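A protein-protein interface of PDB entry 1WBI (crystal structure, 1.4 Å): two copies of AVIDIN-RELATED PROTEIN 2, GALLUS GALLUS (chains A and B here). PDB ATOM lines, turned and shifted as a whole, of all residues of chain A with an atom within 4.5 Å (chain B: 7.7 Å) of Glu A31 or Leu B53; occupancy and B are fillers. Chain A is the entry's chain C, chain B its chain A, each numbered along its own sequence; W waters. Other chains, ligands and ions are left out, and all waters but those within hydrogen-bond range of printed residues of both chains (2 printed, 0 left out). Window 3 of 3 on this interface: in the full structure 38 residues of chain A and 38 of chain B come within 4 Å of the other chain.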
ATOM      1  N   ALA A  25      -0.119  22.726 -23.727  1.00  0.00           N
ATOM      2  CA  ALA A  25      -0.672  22.922 -25.080  1.00  0.00           C
ATOM      3  C   ALA A  25      -1.319  21.641 -25.608  1.00  0.00           C
ATOM      4  O   ALA A  25      -0.771  20.539 -25.433  1.00  0.00           O
ATOM      5  CB  ALA A  25       0.378  23.371 -26.012  1.00  0.00           C
ATOM      6  N   VAL A  26      -2.472  21.808 -26.257  1.00  0.00           N
ATOM      7  CA  VAL A  26      -3.144  20.719 -26.929  1.00  0.00           C
ATOM      8  C   VAL A  26      -2.683  20.727 -28.380  1.00  0.00           C
ATOM      9  O   VAL A  26      -2.827  21.746 -29.081  1.00  0.00           O
ATOM     10  CB  VAL A  26      -4.681  20.877 -26.857  1.00  0.00           C
ATOM     11  CG1 VAL A  26      -5.397  19.763 -27.586  1.00  0.00           C
ATOM     12  CG2 VAL A  26      -5.137  20.934 -25.416  1.00  0.00           C
ATOM     13  N   ASN A  27      -2.144  19.610 -28.839  1.00  0.00           N
ATOM     14  CA  ASN A  27      -1.594  19.568 -30.187  1.00  0.00           C
ATOM     15  C   ASN A  27      -2.669  19.349 -31.261  1.00  0.00           C
ATOM     16  O   ASN A  27      -3.870  19.308 -30.977  1.00  0.00           O
ATOM     17  CB  ASN A  27      -0.402  18.601 -30.270  1.00  0.00           C
ATOM     18  CG  ASN A  27      -0.783  17.106 -30.257  1.00  0.00           C
ATOM     19  OD1 ASN A  27      -1.943  16.699 -30.395  1.00  0.00           O
ATOM     20  ND2 ASN A  27       0.236  16.283 -30.153  1.00  0.00           N
ATOM     21  N   ASN A  29      -3.522  16.828 -32.889  1.00  0.00           N
ATOM     22  CA  ASN A  29      -4.270  15.572 -32.676  1.00  0.00           C
ATOM     23  C   ASN A  29      -5.057  15.531 -31.355  1.00  0.00           C
ATOM     24  O   ASN A  29      -5.645  14.500 -31.001  1.00  0.00           O
ATOM     25  CB  ASN A  29      -3.298  14.413 -32.745  1.00  0.00           C
ATOM     26  CG  ASN A  29      -2.797  14.158 -34.177  1.00  0.00           C
ATOM     27  OD1 ASN A  29      -3.522  14.374 -35.150  1.00  0.00           O
ATOM     28  ND2 ASN A  29      -1.577  13.672 -34.293  1.00  0.00           N
ATOM     29  N   GLY A  30      -5.111  16.665 -30.656  1.00  0.00           N
ATOM     30  CA  GLY A  30      -5.878  16.779 -29.417  1.00  0.00           C
ATOM     31  C   GLY A  30      -5.141  16.253 -28.199  1.00  0.00           C
ATOM     32  O   GLY A  30      -5.750  16.137 -27.134  1.00  0.00           O
ATOM     33  N   GLU A  31      -3.858  15.919 -28.340  1.00  0.00           N
ATOM     34  CA  GLU A  31      -3.080  15.322 -27.251  1.00  0.00           C
ATOM     35  C   GLU A  31      -2.553  16.405 -26.313  1.00  0.00           C
ATOM     36  O   GLU A  31      -2.199  17.518 -26.744  1.00  0.00           O
ATOM     37  CB  GLU A  31      -1.928  14.518 -27.814  1.00  0.00           C
ATOM     38  CG  GLU A  31      -2.337  13.417 -28.807  1.00  0.00           C
ATOM     39  CD  GLU A  31      -1.176  12.878 -29.635  1.00  0.00           C
ATOM     40  OE1 GLU A  31      -0.015  13.311 -29.446  1.00  0.00           O
ATOM     41  OE2 GLU A  31      -1.445  12.027 -30.506  1.00  0.00           O
ATOM     42  N   PHE A  32      -2.505  16.083 -25.024  1.00  0.00           N
ATOM     43  CA  PHE A  32      -1.995  16.996 -24.011  1.00  0.00           C
ATOM     44  C   PHE A  32      -1.386  16.253 -22.844  1.00  0.00           C
ATOM     45  O   PHE A  32      -1.691  15.058 -22.588  1.00  0.00           O
ATOM     46  CB  PHE A  32      -3.082  17.921 -23.490  1.00  0.00           C
ATOM     47  CG  PHE A  32      -4.285  17.203 -22.898  1.00  0.00           C
ATOM     48  CD1 PHE A  32      -4.283  16.790 -21.552  1.00  0.00           C
ATOM     49  CD2 PHE A  32      -5.387  16.881 -23.678  1.00  0.00           C
ATOM     50  CE1 PHE A  32      -5.385  16.101 -21.026  1.00  0.00           C
ATOM     51  CE2 PHE A  32      -6.470  16.236 -23.156  1.00  0.00           C
ATOM     52  CZ  PHE A  32      -6.482  15.836 -21.811  1.00  0.00           C
ATOM     53  N   LEU A  53      -1.606  12.494 -18.912  1.00  0.00           N
ATOM     54  CA  LEU A  53      -1.486  12.465 -20.354  1.00  0.00           C
ATOM     55  C   LEU A  53      -2.862  12.099 -20.905  1.00  0.00           C
ATOM     56  O   LEU A  53      -3.489  11.169 -20.412  1.00  0.00           O
ATOM     57  CB  LEU A  53      -0.478  11.394 -20.723  1.00  0.00           C
ATOM     58  CG  LEU A  53      -0.105  11.274 -22.204  1.00  0.00           C
ATOM     59  CD1 LEU A  53       0.697  12.486 -22.691  1.00  0.00           C
ATOM     60  CD2 LEU A  53       0.743  10.046 -22.418  1.00  0.00           C
ATOM     61  N   GLY A  54      -3.347  12.829 -21.919  1.00  0.00           N
ATOM     62  CA  GLY A  54      -4.709  12.592 -22.405  1.00  0.00           C
ATOM     63  C   GLY A  54      -4.938  13.107 -23.811  1.00  0.00           C
ATOM     64  O   GLY A  54      -4.022  13.607 -24.448  1.00  0.00           O
ATOM     65  N   ILE A  55      -6.181  12.955 -24.264  1.00  0.00           N
ATOM     66  CA  ILE A  55      -6.574  13.385 -25.589  1.00  0.00           C
ATOM     67  C   ILE A  55      -7.962  14.011 -25.488  1.00  0.00           C
ATOM     68  O   ILE A  55      -8.860  13.463 -24.834  1.00  0.00           O
ATOM     69  CB  ILE A  55      -6.654  12.208 -26.612  1.00  0.00           C
ATOM     70  CG1 ILE A  55      -5.515  11.232 -26.458  1.00  0.00           C
ATOM     71  CG2 ILE A  55      -6.707  12.822 -28.051  1.00  0.00           C
ATOM     72  CD1 ILE A  55      -5.593  10.044 -27.395  1.00  0.00           C
ATOM     73  N   GLU B  31       5.178   6.495 -20.584  1.00  0.00           N
ATOM     74  CA  GLU B  31       4.203   6.939 -21.562  1.00  0.00           C
ATOM     75  C   GLU B  31       4.263   6.146 -22.846  1.00  0.00           C
ATOM     76  O   GLU B  31       5.332   5.724 -23.256  1.00  0.00           O
ATOM     77  CB  GLU B  31       4.399   8.418 -21.916  1.00  0.00           C
ATOM     78  CG  GLU B  31       4.393   9.369 -20.716  1.00  0.00           C
ATOM     79  CD  GLU B  31       4.849  10.781 -21.093  1.00  0.00           C
ATOM     80  OE1 GLU B  31       5.593  10.925 -22.103  1.00  0.00           O
ATOM     81  OE2 GLU B  31       4.464  11.740 -20.372  1.00  0.00           O
ATOM     82  N   PHE B  32       3.108   5.947 -23.457  1.00  0.00           N
ATOM     83  CA  PHE B  32       3.009   5.193 -24.709  1.00  0.00           C
ATOM     84  C   PHE B  32       1.841   5.678 -25.531  1.00  0.00           C
ATOM     85  O   PHE B  32       0.899   6.256 -25.017  1.00  0.00           O
ATOM     86  CB  PHE B  32       2.905   3.694 -24.442  1.00  0.00           C
ATOM     87  CG  PHE B  32       1.711   3.307 -23.591  1.00  0.00           C
ATOM     88  CD1 PHE B  32       0.462   3.070 -24.166  1.00  0.00           C
ATOM     89  CD2 PHE B  32       1.837   3.208 -22.216  1.00  0.00           C
ATOM     90  CE1 PHE B  32      -0.661   2.752 -23.376  1.00  0.00           C
ATOM     91  CE2 PHE B  32       0.742   2.870 -21.418  1.00  0.00           C
ATOM     92  CZ  PHE B  32      -0.509   2.656 -21.986  1.00  0.00           C
ATOM     93  N   ASP B  33       1.913   5.378 -26.826  1.00  0.00           N
ATOM     94  CA  ASP B  33       0.883   5.631 -27.786  1.00  0.00           C
ATOM     95  C   ASP B  33       0.596   4.347 -28.521  1.00  0.00           C
ATOM     96  O   ASP B  33       1.301   3.353 -28.389  1.00  0.00           O
ATOM     97  CB  ASP B  33       1.250   6.802 -28.720  1.00  0.00           C
ATOM     98  CG  ASP B  33       2.497   6.534 -29.539  1.00  0.00           C
ATOM     99  OD1 ASP B  33       2.489   5.589 -30.328  1.00  0.00           O
ATOM    100  OD2 ASP B  33       3.497   7.256 -29.365  1.00  0.00           O
ATOM    101  N   GLY B  34      -0.469   4.331 -29.278  1.00  0.00           N
ATOM    102  CA  GLY B  34      -0.801   3.153 -30.043  1.00  0.00           C
ATOM    103  C   GLY B  34      -2.062   3.394 -30.851  1.00  0.00           C
ATOM    104  O   GLY B  34      -2.571   4.532 -30.950  1.00  0.00           O
ATOM    105  N   THR B  35      -2.573   2.307 -31.407  1.00  0.00           N
ATOM    106  CA  THR B  35      -3.773   2.286 -32.227  1.00  0.00           C
ATOM    107  C   THR B  35      -4.715   1.201 -31.725  1.00  0.00           C
ATOM    108  O   THR B  35      -4.284   0.075 -31.439  1.00  0.00           O
ATOM    109  CB  THR B  35      -3.427   1.986 -33.708  1.00  0.00           C
ATOM    110  OG1 THR B  35      -2.567   3.031 -34.193  1.00  0.00           O
ATOM    111  CG2 THR B  35      -4.698   1.885 -34.556  1.00  0.00           C
ATOM    112  N   SER B  50      -8.302   3.984 -34.315  1.00  0.00           N
ATOM    113  CA  SER B  50      -8.347   5.169 -33.492  1.00  0.00           C
ATOM    114  C   SER B  50      -7.158   5.197 -32.571  1.00  0.00           C
ATOM    115  O   SER B  50      -6.715   4.134 -32.097  1.00  0.00           O
ATOM    116  CB  SER B  50      -9.641   5.235 -32.666  1.00  0.00           C
ATOM    117  OG  SER B  50     -10.812   5.271 -33.436  1.00  0.00           O
ATOM    118  N   PRO B  51      -6.614   6.392 -32.324  1.00  0.00           N
ATOM    119  CA  PRO B  51      -5.409   6.582 -31.533  1.00  0.00           C
ATOM    120  C   PRO B  51      -5.645   6.440 -30.017  1.00  0.00           C
ATOM    121  O   PRO B  51      -6.695   6.835 -29.503  1.00  0.00           O
ATOM    122  CB  PRO B  51      -4.992   8.027 -31.874  1.00  0.00           C
ATOM    123  CG  PRO B  51      -6.218   8.686 -32.179  1.00  0.00           C
ATOM    124  CD  PRO B  51      -7.120   7.671 -32.835  1.00  0.00           C
ATOM    125  N   LEU B  52      -4.649   5.890 -29.343  1.00  0.00           N
ATOM    126  CA  LEU B  52      -4.642   5.875 -27.903  1.00  0.00           C
ATOM    127  C   LEU B  52      -3.359   6.482 -27.357  1.00  0.00           C
ATOM    128  O   LEU B  52      -2.312   6.567 -28.047  1.00  0.00           O
ATOM    129  CB  LEU B  52      -4.845   4.468 -27.390  1.00  0.00           C
ATOM    130  CG  LEU B  52      -3.669   3.497 -27.555  1.00  0.00           C
ATOM    131  CD1 LEU B  52      -2.756   3.502 -26.372  1.00  0.00           C
ATOM    132  CD2 LEU B  52      -4.125   2.098 -27.828  1.00  0.00           C
ATOM    133  N   LEU B  53      -3.399   6.888 -26.088  1.00  0.00           N
ATOM    134  CA  LEU B  53      -2.268   7.465 -25.397  1.00  0.00           C
ATOM    135  C   LEU B  53      -2.419   7.127 -23.931  1.00  0.00           C
ATOM    136  O   LEU B  53      -3.523   7.295 -23.399  1.00  0.00           O
ATOM    137  CB  LEU B  53      -2.335   8.968 -25.550  1.00  0.00           C
ATOM    138  CG  LEU B  53      -1.159   9.824 -25.212  1.00  0.00           C
ATOM    139  CD1 LEU B  53       0.049   9.380 -26.042  1.00  0.00           C
ATOM    140  CD2 LEU B  53      -1.494  11.316 -25.461  1.00  0.00           C
ATOM    141  N   GLY B  54      -1.358   6.655 -23.276  1.00  0.00           N
ATOM    142  CA  GLY B  54      -1.468   6.312 -21.864  1.00  0.00           C
ATOM    143  C   GLY B  54      -0.180   6.284 -21.112  1.00  0.00           C
ATOM    144  O   GLY B  54       0.867   6.646 -21.637  1.00  0.00           O
ATOM    145  N   ILE B  55      -0.265   5.846 -19.858  1.00  0.00           N
ATOM    146  CA  ILE B  55       0.919   5.735 -19.007  1.00  0.00           C
ATOM    147  C   ILE B  55       0.849   4.470 -18.198  1.00  0.00           C
ATOM    148  O   ILE B  55      -0.221   4.115 -17.705  1.00  0.00           O
ATOM    149  CB  ILE B  55       1.073   6.925 -18.025  1.00  0.00           C
ATOM    150  CG1 ILE B  55       0.685   8.263 -18.645  1.00  0.00           C
ATOM    151  CG2 ILE B  55       2.502   6.977 -17.470  1.00  0.00           C
ATOM    152  CD1 ILE B  55       0.629   9.393 -17.625  1.00  0.00           C
ATOM    153  N   GLY B  66      -3.008   3.046 -17.425  1.00  0.00           N
ATOM    154  CA  GLY B  66      -4.236   3.603 -17.958  1.00  0.00           C
ATOM    155  C   GLY B  66      -4.007   4.128 -19.359  1.00  0.00           C
ATOM    156  O   GLY B  66      -2.842   4.455 -19.730  1.00  0.00           O
ATOM    157  N   PHE B  67      -5.071   4.190 -20.164  1.00  0.00           N
ATOM    158  CA  PHE B  67      -5.000   4.881 -21.433  1.00  0.00           C
ATOM    159  C   PHE B  67      -6.329   5.450 -21.860  1.00  0.00           C
ATOM    160  O   PHE B  67      -7.372   5.006 -21.408  1.00  0.00           O
ATOM    161  CB  PHE B  67      -4.368   4.007 -22.545  1.00  0.00           C
ATOM    162  CG  PHE B  67      -5.105   2.729 -22.850  1.00  0.00           C
ATOM    163  CD1 PHE B  67      -6.065   2.671 -23.827  1.00  0.00           C
ATOM    164  CD2 PHE B  67      -4.760   1.551 -22.211  1.00  0.00           C
ATOM    165  CE1 PHE B  67      -6.731   1.494 -24.114  1.00  0.00           C
ATOM    166  CE2 PHE B  67      -5.421   0.363 -22.476  1.00  0.00           C
ATOM    167  CZ  PHE B  67      -6.378   0.317 -23.485  1.00  0.00           C
ATOM    168  N   THR B  68      -6.243   6.407 -22.777  1.00  0.00           N
ATOM    169  CA  THR B  68      -7.379   7.094 -23.395  1.00  0.00           C
ATOM    170  C   THR B  68      -7.430   6.705 -24.861  1.00  0.00           C
ATOM    171  O   THR B  68      -6.369   6.651 -25.518  1.00  0.00           O
ATOM    172  CB  THR B  68      -7.248   8.613 -23.312  1.00  0.00           C
ATOM    173  OG1 THR B  68      -7.216   9.036 -21.921  1.00  0.00           O
ATOM    174  CG2 THR B  68      -8.382   9.303 -23.939  1.00  0.00           C
ATOM    175  N   VAL B  69      -8.624   6.378 -25.357  1.00  0.00           N
ATOM    176  CA  VAL B  69      -8.847   6.234 -26.798  1.00  0.00           C
ATOM    177  C   VAL B  69      -9.737   7.347 -27.306  1.00  0.00           C
ATOM    178  O   VAL B  69     -10.863   7.536 -26.866  1.00  0.00           O
ATOM    179  CB  VAL B  69      -9.501   4.881 -27.120  1.00  0.00           C
ATOM    180  CG1 VAL B  69      -9.654   4.684 -28.631  1.00  0.00           C
ATOM    181  CG2 VAL B  69      -8.767   3.739 -26.486  1.00  0.00           C
ATOM    182  N   HIS B  70      -9.229   8.064 -28.293  1.00  0.00           N
ATOM    183  CA  HIS B  70      -9.970   9.132 -28.999  1.00  0.00           C
ATOM    184  C   HIS B  70     -10.565   8.508 -30.242  1.00  0.00           C
ATOM    185  O   HIS B  70      -9.832   8.229 -31.197  1.00  0.00           O
ATOM    186  CB  HIS B  70      -8.999  10.293 -29.368  1.00  0.00           C
ATOM    187  CG  HIS B  70      -9.549  11.260 -30.374  1.00  0.00           C
ATOM    188  ND1 HIS B  70      -9.746  10.936 -31.704  1.00  0.00           N
ATOM    189  CD2 HIS B  70      -9.964  12.545 -30.232  1.00  0.00           C
ATOM    190  CE1 HIS B  70     -10.238  11.991 -32.334  1.00  0.00           C
ATOM    191  NE2 HIS B  70     -10.355  12.988 -31.476  1.00  0.00           N
ATOM    192  N   SER B  78     -13.107   6.956 -24.811  1.00  0.00           N
ATOM    193  CA  SER B  78     -13.063   5.912 -23.772  1.00  0.00           C
ATOM    194  C   SER B  78     -11.758   5.981 -22.994  1.00  0.00           C
ATOM    195  O   SER B  78     -10.758   6.396 -23.524  1.00  0.00           O
ATOM    196  CB  SER B  78     -13.192   4.523 -24.363  1.00  0.00           C
ATOM    197  OG  SER B  78     -14.505   4.346 -24.913  1.00  0.00           O
ATOM    198  N   VAL B  79     -11.803   5.563 -21.722  1.00  0.00           N
ATOM    199  CA  VAL B  79     -10.599   5.353 -20.928  1.00  0.00           C
ATOM    200  C   VAL B  79     -10.629   3.973 -20.309  1.00  0.00           C
ATOM    201  O   VAL B  79     -11.715   3.417 -19.984  1.00  0.00           O
ATOM    202  CB  VAL B  79     -10.439   6.389 -19.809  1.00  0.00           C
ATOM    203  CG1 VAL B  79     -10.240   7.834 -20.357  1.00  0.00           C
ATOM    204  CG2 VAL B  79     -11.667   6.397 -18.898  1.00  0.00           C
ATOM    205  N   PHE B  80      -9.442   3.374 -20.243  1.00  0.00           N
ATOM    206  CA  PHE B  80      -9.215   2.053 -19.669  1.00  0.00           C
ATOM    207  C   PHE B  80      -8.211   2.166 -18.548  1.00  0.00           C
ATOM    208  O   PHE B  80      -7.195   2.854 -18.682  1.00  0.00           O
ATOM    209  CB  PHE B  80      -8.639   1.110 -20.752  1.00  0.00           C
ATOM    210  CG  PHE B  80      -9.578   0.759 -21.896  1.00  0.00           C
ATOM    211  CD1 PHE B  80     -10.183  -0.458 -21.930  1.00  0.00           C
ATOM    212  CD2 PHE B  80      -9.874   1.678 -22.892  1.00  0.00           C
ATOM    213  CE1 PHE B  80     -11.042  -0.794 -23.009  1.00  0.00           C
ATOM    214  CE2 PHE B  80     -10.757   1.329 -23.943  1.00  0.00           C
ATOM    215  CZ  PHE B  80     -11.328   0.139 -23.950  1.00  0.00           C
HETATM  216  O   HOH W   1      -4.480   8.798 -21.309  1.00  0.00           O
HETATM  217  O   HOH W   2      -8.418  15.633 -31.474  1.00  0.00           O
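The backbone carbonyl oxygen (O) of Phe A32 lies within hydrogen-bond range of the backbone NH (N) of Gly A54 (2.9 Å).
OD1 of Asn A27 is in hydrogen-bond range of N of Glu A31 (2.9 Å).
The backbone NH (N) of Gly B54 lies within hydrogen-bond range of the backbone carbonyl oxygen (O) of Phe B32 (2.9 Å).
The backbone NH (N) of Ile B55 lies within hydrogen-bond range of the backbone carbonyl oxygen (O) of Gly B66 (2.9 Å).
The backbone carbonyl oxygen (O) of Leu B53 lies within hydrogen-bond range of the backbone NH (N) of Thr B68, 2.9 Å away.
The backbone carbonyl oxygen (O) of Pro B51 is in hydrogen-bond range of the backbone NH (N) of His B70 (3.1 Å).
Among the printed residues, merely in contact across the chains: Leu A53 with Leu B53 (3.4 Å), Leu A53 with Gly B54 (3.5 Å), Gly A54 with Leu B53 (3.6 Å), Ile A55 with His B70 (3.7 Å), Leu A53 with Ile B55 (3.9 Å), Ile A55 with Leu B53 (3.9 Å), Ile A55 with Thr B68 (3.95 Å), Ile A55 with Pro B51 (3.99 Å) and Glu A31 with Leu B53 (3.997 Å).
Printed residues of chain B within 4 Å of Glu A31: Leu B53.
Printed residues of chain A within 4 Å of Leu B53: Glu A31 (3.997 Å), Leu A53 (3.4 Å), Gly A54 (3.6 Å) and Ile A55 (3.9 Å).
No residue of chain B comes within 4 Å of Gly A30.
Printed residues of chain A within 4 Å of Ile B55: Leu A53.
Of the printed residues of chain A, His B70 touches Ile A55.
Of the printed residues of chain B, Gly A54 touches Leu B53.
Phe B80 touches none of the printed residues of chain A.
The nearest printed residue of chain B that does not touch Glu A31 is Pro B51 (5.5 Å).
Hydrophobic or aromatic side chains of chain B that line the printed part of chain A: Leu B53, Ile B55 and His B70.
Hydrophobic or aromatic side chains of chain A within 4 Å of the printed part of chain B: Leu A53 and Ile A55.
Among the printed residues, 9 pairs touch across the chains.
Among the printed residues, no Asp or Glu carboxylate lies within 4 Å of a Lys or Arg side-chain nitrogen of the other chain.
Glu A31 touches Leu B53, but with the chains exchanged Leu A53 does not touch Glu B31 (4.03 Å).
Leu A53 touches its own counterpart, Leu B53.
Leu A53 touches Gly B54, and with the chains exchanged Gly A54 touches Leu B53.
Leu A53 touches Ile B55, and with the chains exchanged Ile A55 touches Leu B53.
Positions printed for both chains: 31, 32, 53, 54 and 55.
Water W1 lies within hydrogen-bond range of O of Leu A53 (2.7 Å), O of Leu B53 (2.7 Å) and OG1 of Thr B68 (2.8 Å).
Water W2 lies within hydrogen-bond range of O of Asn A29 and NE2 of His B70.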
